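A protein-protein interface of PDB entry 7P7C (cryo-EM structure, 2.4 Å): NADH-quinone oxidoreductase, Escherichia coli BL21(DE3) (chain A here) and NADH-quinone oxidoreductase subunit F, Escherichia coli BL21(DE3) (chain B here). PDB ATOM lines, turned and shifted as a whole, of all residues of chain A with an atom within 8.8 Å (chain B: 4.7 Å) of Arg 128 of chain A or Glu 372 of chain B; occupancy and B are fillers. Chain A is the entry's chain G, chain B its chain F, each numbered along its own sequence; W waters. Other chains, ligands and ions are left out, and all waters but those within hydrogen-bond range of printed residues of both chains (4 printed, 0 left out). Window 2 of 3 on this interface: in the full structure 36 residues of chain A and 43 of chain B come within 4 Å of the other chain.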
ATOM      1  N   GLU A  92       8.464  26.338   0.897  1.00  0.00           N
ATOM      2  CA  GLU A  92       8.341  25.839   2.264  1.00  0.00           C
ATOM      3  C   GLU A  92       8.001  26.953   3.249  1.00  0.00           C
ATOM      4  O   GLU A  92       7.194  26.754   4.162  1.00  0.00           O
ATOM      5  CB  GLU A  92       9.635  25.141   2.678  1.00  0.00           C
ATOM      6  CG  GLU A  92       9.588  24.546   4.067  1.00  0.00           C
ATOM      7  CD  GLU A  92      10.828  23.756   4.410  1.00  0.00           C
ATOM      8  OE1 GLU A  92      11.857  23.925   3.728  1.00  0.00           O
ATOM      9  OE2 GLU A  92      10.773  22.959   5.364  1.00  0.00           O
ATOM     10  N   THR A  96       4.476  27.286   5.708  1.00  0.00           N
ATOM     11  CA  THR A  96       4.487  27.166   7.164  1.00  0.00           C
ATOM     12  C   THR A  96       3.176  27.644   7.777  1.00  0.00           C
ATOM     13  O   THR A  96       2.656  27.014   8.702  1.00  0.00           O
ATOM     14  CB  THR A  96       5.662  27.941   7.763  1.00  0.00           C
ATOM     15  OG1 THR A  96       5.653  29.287   7.276  1.00  0.00           O
ATOM     16  CG2 THR A  96       6.979  27.285   7.405  1.00  0.00           C
ATOM     17  N   ARG A 125       6.800  18.116   5.146  1.00  0.00           N
ATOM     18  CA  ARG A 125       6.698  19.189   6.128  1.00  0.00           C
ATOM     19  C   ARG A 125       7.563  18.854   7.335  1.00  0.00           C
ATOM     20  O   ARG A 125       7.402  17.792   7.943  1.00  0.00           O
ATOM     21  CB  ARG A 125       5.246  19.396   6.557  1.00  0.00           C
ATOM     22  CG  ARG A 125       5.010  20.600   7.460  1.00  0.00           C
ATOM     23  CD  ARG A 125       3.538  20.712   7.827  1.00  0.00           C
ATOM     24  NE  ARG A 125       3.233  21.877   8.648  1.00  0.00           N
ATOM     25  CZ  ARG A 125       3.027  23.100   8.175  1.00  0.00           C
ATOM     26  NH1 ARG A 125       3.137  23.370   6.887  1.00  0.00           N
ATOM     27  NH2 ARG A 125       2.711  24.076   9.018  1.00  0.00           N
ATOM     28  N   ARG A 126       8.477  19.758   7.678  1.00  0.00           N
ATOM     29  CA  ARG A 126       9.248  19.651   8.906  1.00  0.00           C
ATOM     30  C   ARG A 126       8.944  20.765   9.892  1.00  0.00           C
ATOM     31  O   ARG A 126       9.382  20.687  11.044  1.00  0.00           O
ATOM     32  CB  ARG A 126      10.751  19.637   8.598  1.00  0.00           C
ATOM     33  CG  ARG A 126      11.109  20.391   7.353  1.00  0.00           C
ATOM     34  CD  ARG A 126      12.591  20.344   7.051  1.00  0.00           C
ATOM     35  NE  ARG A 126      12.933  21.376   6.083  1.00  0.00           N
ATOM     36  CZ  ARG A 126      13.801  22.353   6.299  1.00  0.00           C
ATOM     37  NH1 ARG A 126      14.487  22.431   7.426  1.00  0.00           N
ATOM     38  NH2 ARG A 126      13.981  23.277   5.362  1.00  0.00           N
ATOM     39  N   TYR A 127       8.222  21.797   9.468  1.00  0.00           N
ATOM     40  CA  TYR A 127       7.725  22.814  10.382  1.00  0.00           C
ATOM     41  C   TYR A 127       6.707  22.195  11.329  1.00  0.00           C
ATOM     42  O   TYR A 127       5.803  21.474  10.898  1.00  0.00           O
ATOM     43  CB  TYR A 127       7.102  23.957   9.582  1.00  0.00           C
ATOM     44  CG  TYR A 127       6.635  25.142  10.389  1.00  0.00           C
ATOM     45  CD1 TYR A 127       7.520  26.137  10.776  1.00  0.00           C
ATOM     46  CD2 TYR A 127       5.300  25.281  10.739  1.00  0.00           C
ATOM     47  CE1 TYR A 127       7.090  27.226  11.499  1.00  0.00           C
ATOM     48  CE2 TYR A 127       4.864  26.363  11.460  1.00  0.00           C
ATOM     49  CZ  TYR A 127       5.761  27.331  11.840  1.00  0.00           C
ATOM     50  OH  TYR A 127       5.323  28.411  12.560  1.00  0.00           O
ATOM     51  N   ARG A 128       6.853  22.469  12.624  1.00  0.00           N
ATOM     52  CA  ARG A 128       5.998  21.858  13.630  1.00  0.00           C
ATOM     53  C   ARG A 128       5.308  22.860  14.539  1.00  0.00           C
ATOM     54  O   ARG A 128       4.619  22.445  15.476  1.00  0.00           O
ATOM     55  CB  ARG A 128       6.808  20.882  14.495  1.00  0.00           C
ATOM     56  CG  ARG A 128       7.776  21.567  15.435  1.00  0.00           C
ATOM     57  CD  ARG A 128       8.403  20.580  16.391  1.00  0.00           C
ATOM     58  NE  ARG A 128       9.264  21.236  17.366  1.00  0.00           N
ATOM     59  CZ  ARG A 128      10.525  21.579  17.142  1.00  0.00           C
ATOM     60  NH1 ARG A 128      11.105  21.354  15.976  1.00  0.00           N
ATOM     61  NH2 ARG A 128      11.219  22.163  18.113  1.00  0.00           N
ATOM     62  N   PHE A 129       5.464  24.152  14.297  1.00  0.00           N
ATOM     63  CA  PHE A 129       4.956  25.163  15.205  1.00  0.00           C
ATOM     64  C   PHE A 129       3.578  25.631  14.743  1.00  0.00           C
ATOM     65  O   PHE A 129       2.975  25.060  13.832  1.00  0.00           O
ATOM     66  CB  PHE A 129       5.966  26.298  15.316  1.00  0.00           C
ATOM     67  CG  PHE A 129       7.346  25.839  15.689  1.00  0.00           C
ATOM     68  CD1 PHE A 129       7.650  25.511  16.999  1.00  0.00           C
ATOM     69  CD2 PHE A 129       8.337  25.727  14.731  1.00  0.00           C
ATOM     70  CE1 PHE A 129       8.916  25.086  17.347  1.00  0.00           C
ATOM     71  CE2 PHE A 129       9.605  25.300  15.072  1.00  0.00           C
ATOM     72  CZ  PHE A 129       9.894  24.981  16.383  1.00  0.00           C
ATOM     73  N   THR A 130       3.057  26.675  15.379  1.00  0.00           N
ATOM     74  CA  THR A 130       1.703  27.126  15.103  1.00  0.00           C
ATOM     75  C   THR A 130       1.648  27.934  13.813  1.00  0.00           C
ATOM     76  O   THR A 130       2.641  28.515  13.371  1.00  0.00           O
ATOM     77  CB  THR A 130       1.164  27.965  16.260  1.00  0.00           C
ATOM     78  OG1 THR A 130       2.004  29.107  16.460  1.00  0.00           O
ATOM     79  CG2 THR A 130       1.123  27.141  17.533  1.00  0.00           C
ATOM     80  N   LYS A 131       0.466  27.960  13.209  1.00  0.00           N
ATOM     81  CA  LYS A 131       0.217  28.725  11.999  1.00  0.00           C
ATOM     82  C   LYS A 131      -0.552  29.990  12.346  1.00  0.00           C
ATOM     83  O   LYS A 131      -1.503  29.952  13.130  1.00  0.00           O
ATOM     84  CB  LYS A 131      -0.571  27.901  10.980  1.00  0.00           C
ATOM     85  CG  LYS A 131       0.019  26.539  10.693  1.00  0.00           C
ATOM     86  CD  LYS A 131      -0.457  26.010   9.356  1.00  0.00           C
ATOM     87  CE  LYS A 131      -1.047  24.625   9.484  1.00  0.00           C
ATOM     88  NZ  LYS A 131      -2.409  24.658  10.071  1.00  0.00           N
ATOM     89  N   ALA B 367      12.037  27.241  21.368  1.00  0.00           N
ATOM     90  CA  ALA B 367      12.055  25.835  21.759  1.00  0.00           C
ATOM     91  C   ALA B 367      13.404  25.433  22.347  1.00  0.00           C
ATOM     92  O   ALA B 367      13.462  24.638  23.291  1.00  0.00           O
ATOM     93  CB  ALA B 367      11.708  24.954  20.561  1.00  0.00           C
ATOM     94  N   ARG B 370      13.705  26.765  25.933  1.00  0.00           N
ATOM     95  CA  ARG B 370      12.868  26.008  26.853  1.00  0.00           C
ATOM     96  C   ARG B 370      13.301  24.557  26.998  1.00  0.00           C
ATOM     97  O   ARG B 370      12.701  23.828  27.792  1.00  0.00           O
ATOM     98  CB  ARG B 370      11.410  26.055  26.395  1.00  0.00           C
ATOM     99  CG  ARG B 370      10.690  27.346  26.724  1.00  0.00           C
ATOM    100  CD  ARG B 370       9.284  27.351  26.150  1.00  0.00           C
ATOM    101  NE  ARG B 370       9.142  26.429  25.029  1.00  0.00           N
ATOM    102  CZ  ARG B 370       8.694  26.773  23.829  1.00  0.00           C
ATOM    103  NH1 ARG B 370       8.326  28.013  23.557  1.00  0.00           N
ATOM    104  NH2 ARG B 370       8.613  25.848  22.877  1.00  0.00           N
ATOM    105  N   GLY B 371      14.317  24.121  26.261  1.00  0.00           N
ATOM    106  CA  GLY B 371      14.711  22.730  26.294  1.00  0.00           C
ATOM    107  C   GLY B 371      13.810  21.803  25.517  1.00  0.00           C
ATOM    108  O   GLY B 371      13.811  20.595  25.773  1.00  0.00           O
ATOM    109  N   GLU B 372      13.032  22.332  24.574  1.00  0.00           N
ATOM    110  CA  GLU B 372      12.145  21.538  23.738  1.00  0.00           C
ATOM    111  C   GLU B 372      12.645  21.458  22.299  1.00  0.00           C
ATOM    112  O   GLU B 372      11.853  21.298  21.368  1.00  0.00           O
ATOM    113  CB  GLU B 372      10.727  22.102  23.776  1.00  0.00           C
ATOM    114  CG  GLU B 372      10.045  21.960  25.119  1.00  0.00           C
ATOM    115  CD  GLU B 372       9.036  23.059  25.374  1.00  0.00           C
ATOM    116  OE1 GLU B 372       8.534  23.646  24.393  1.00  0.00           O
ATOM    117  OE2 GLU B 372       8.743  23.336  26.556  1.00  0.00           O
ATOM    118  N   GLY B 373      13.955  21.584  22.105  1.00  0.00           N
ATOM    119  CA  GLY B 373      14.512  21.446  20.778  1.00  0.00           C
ATOM    120  C   GLY B 373      14.457  20.013  20.288  1.00  0.00           C
ATOM    121  O   GLY B 373      14.428  19.060  21.065  1.00  0.00           O
ATOM    122  N   GLN B 374      14.439  19.867  18.973  1.00  0.00           N
ATOM    123  CA  GLN B 374      14.316  18.589  18.295  1.00  0.00           C
ATOM    124  C   GLN B 374      15.415  18.489  17.250  1.00  0.00           C
ATOM    125  O   GLN B 374      15.965  19.512  16.828  1.00  0.00           O
ATOM    126  CB  GLN B 374      12.929  18.456  17.647  1.00  0.00           C
ATOM    127  CG  GLN B 374      11.801  18.436  18.667  1.00  0.00           C
ATOM    128  CD  GLN B 374      10.448  18.188  18.051  1.00  0.00           C
ATOM    129  OE1 GLN B 374      10.337  17.939  16.855  1.00  0.00           O
ATOM    130  NE2 GLN B 374       9.406  18.259  18.866  1.00  0.00           N
ATOM    131  N   ASP B 377      16.803  21.056  14.096  1.00  0.00           N
ATOM    132  CA  ASP B 377      16.526  22.467  14.353  1.00  0.00           C
ATOM    133  C   ASP B 377      17.742  23.340  14.072  1.00  0.00           C
ATOM    134  O   ASP B 377      17.614  24.418  13.479  1.00  0.00           O
ATOM    135  CB  ASP B 377      16.054  22.652  15.793  1.00  0.00           C
ATOM    136  CG  ASP B 377      14.563  22.438  15.949  1.00  0.00           C
ATOM    137  OD1 ASP B 377      13.870  22.305  14.920  1.00  0.00           O
ATOM    138  OD2 ASP B 377      14.081  22.406  17.099  1.00  0.00           O
ATOM    139  N   GLY B 419      19.818  22.617  23.975  1.00  0.00           N
ATOM    140  CA  GLY B 419      18.378  22.791  23.934  1.00  0.00           C
ATOM    141  C   GLY B 419      17.624  21.656  23.281  1.00  0.00           C
ATOM    142  O   GLY B 419      16.409  21.551  23.467  1.00  0.00           O
ATOM    143  N   GLN B 422      14.236  16.460  22.942  1.00  0.00           N
ATOM    144  CA  GLN B 422      13.153  15.556  22.590  1.00  0.00           C
ATOM    145  C   GLN B 422      13.310  15.105  21.146  1.00  0.00           C
ATOM    146  O   GLN B 422      13.878  15.834  20.329  1.00  0.00           O
ATOM    147  CB  GLN B 422      11.781  16.222  22.783  1.00  0.00           C
ATOM    148  CG  GLN B 422      11.789  17.728  22.774  1.00  0.00           C
ATOM    149  CD  GLN B 422      10.427  18.302  23.105  1.00  0.00           C
ATOM    150  OE1 GLN B 422       9.704  18.764  22.224  1.00  0.00           O
ATOM    151  NE2 GLN B 422      10.068  18.274  24.382  1.00  0.00           N
ATOM    152  N   PHE B 424      12.294  14.209  17.218  1.00  0.00           N
ATOM    153  CA  PHE B 424      11.500  14.951  16.251  1.00  0.00           C
ATOM    154  C   PHE B 424      10.120  14.326  16.105  1.00  0.00           C
ATOM    155  O   PHE B 424       9.988  13.117  15.893  1.00  0.00           O
ATOM    156  CB  PHE B 424      12.196  15.001  14.894  1.00  0.00           C
ATOM    157  CG  PHE B 424      11.421  15.758  13.852  1.00  0.00           C
ATOM    158  CD1 PHE B 424      11.343  17.141  13.900  1.00  0.00           C
ATOM    159  CD2 PHE B 424      10.757  15.090  12.837  1.00  0.00           C
ATOM    160  CE1 PHE B 424      10.625  17.844  12.952  1.00  0.00           C
ATOM    161  CE2 PHE B 424      10.038  15.788  11.884  1.00  0.00           C
ATOM    162  CZ  PHE B 424       9.971  17.166  11.941  1.00  0.00           C
ATOM    163  N   SER B 425       9.089  15.158  16.217  1.00  0.00           N
ATOM    164  CA  SER B 425       7.713  14.700  16.068  1.00  0.00           C
ATOM    165  C   SER B 425       6.919  15.815  15.408  1.00  0.00           C
ATOM    166  O   SER B 425       6.713  16.872  16.009  1.00  0.00           O
ATOM    167  CB  SER B 425       7.107  14.316  17.413  1.00  0.00           C
ATOM    168  OG  SER B 425       5.767  13.891  17.255  1.00  0.00           O
ATOM    169  N   ASN B 426       6.484  15.576  14.175  1.00  0.00           N
ATOM    170  CA  ASN B 426       5.627  16.501  13.454  1.00  0.00           C
ATOM    171  C   ASN B 426       4.218  15.969  13.244  1.00  0.00           C
ATOM    172  O   ASN B 426       3.309  16.761  12.984  1.00  0.00           O
ATOM    173  CB  ASN B 426       6.241  16.833  12.087  1.00  0.00           C
ATOM    174  CG  ASN B 426       5.861  18.204  11.601  1.00  0.00           C
ATOM    175  OD1 ASN B 426       5.155  18.939  12.286  1.00  0.00           O
ATOM    176  ND2 ASN B 426       6.324  18.559  10.411  1.00  0.00           N
HETATM  177  O   HOH W   1       3.072  19.616  14.587  1.00  0.00           O
HETATM  178  O   HOH W   2       3.201  20.787  11.229  1.00  0.00           O
HETATM  179  O   HOH W   3       9.030  22.093  20.428  1.00  0.00           O
HETATM  180  O   HOH W   4      13.204  19.928  13.757  1.00  0.00           O
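Phe 424 of chain B touches Arg 126 of chain A (CE1 to O, 3.6 Å). Arg 126 of chain A touches Asn 426 of chain B. CB of Ala 367 of chain B touches NH2 of Arg 128 of chain A, 3.7 Å away. Asn 426 of chain B touches Arg 128 of chain A.
Of the 12 printed residues of chain B, 6 touch a printed residue of chain A. Among the printed residues, 9 pairs touch across the chains.
The backbone carbonyl oxygen (O) of Ala 367 of chain B is in hydrogen-bond range of the backbone NH (N) of Glu 372 of chain B. The guanidinium group of Arg 370 of chain B lies within salt-bridge range of the side-chain carboxylate of Glu 372 of chain B (2.7 Å). The backbone carbonyl oxygen of Glu 372 of chain B sits close to the side-chain amide oxygen of Gln 422 of chain B, 3.4 Å away. The side-chain amide oxygen (OE1) of Gln 374 of chain B is in hydrogen-bond range of the backbone NH (N) of Ser 425 of chain B. The side-chain carboxylate (OE1) of Glu 92 of chain A lies within salt-bridge range of the guanidinium group (NH2) of Arg 126 of chain A, at 2.8 Å. The backbone carbonyl oxygen (O) of Thr 130 of chain A sits at hydrogen-bond distance from the side-chain hydroxyl (OH) of Tyr 127 of chain A (2.8 Å).
The backbone carbonyl oxygen of Glu 372 of chain B sits at hydrogen-bond distance from the guanidinium group of Arg 128 of chain A. The side-chain amide nitrogen of Gln 374 of chain B sits close to the guanidinium group of Arg 128 of chain A, 3.3 Å away. The side-chain carboxylate of Asp 377 of chain B is in salt-bridge range of the guanidinium group of Arg 128 of chain A (3.0 Å). ND2 of Asn 426 of chain B is in hydrogen-bond range of O of Arg 125 of chain A (2.8 Å). OD1 of Asn 426 of chain B lies close to O of Tyr 127 of chain A (3.0 Å).
Water W2 lies within hydrogen-bond range of O of Tyr 127 of chain A, NE of Arg 125 of chain A and OD1 of Asn 426 of chain B. Water W4 lies within hydrogen-bond range of the side-chain carboxylate (OD1) of Asp 377 of chain B and the guanidinium group (NH1) of Arg 128 of chain A. Water W3 bridges O of Glu 372 of chain B (3.1 Å) and NH2 of Arg 128 of chain A (3.2 Å). Water W1 lies within hydrogen-bond range of OD1 of Asn 426 of chain B and O of Arg 128 of chain A.
Of the printed residues of chain B, Arg 128 of chain A touches Ala 367 (3.7 Å), Glu 372 (3.4 Å), Gln 374 (3.3 Å), Asp 377 (3.0 Å) and Asn 426 (3.3 Å). Of the printed residues of chain A, Ala 367 of chain B touches Arg 128 (3.7 Å). Arg 370 of chain B touches none of the printed residues of chain A. No residue of chain A comes within 4 Å of Gly 371 of chain B. Printed residues of chain A within 4 Å of Glu 372 of chain B: Arg 128 (3.4 Å). No residue of chain A comes within 4 Å of Gly 373 of chain B. Gly 419 of chain B touches none of the printed residues of chain A. Of the printed residues of chain A, Phe 424 of chain B touches Arg 126. The nearest residue of chain B that does not touch Arg 128 of chain A is Ser 425 of chain B (4.1 Å).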
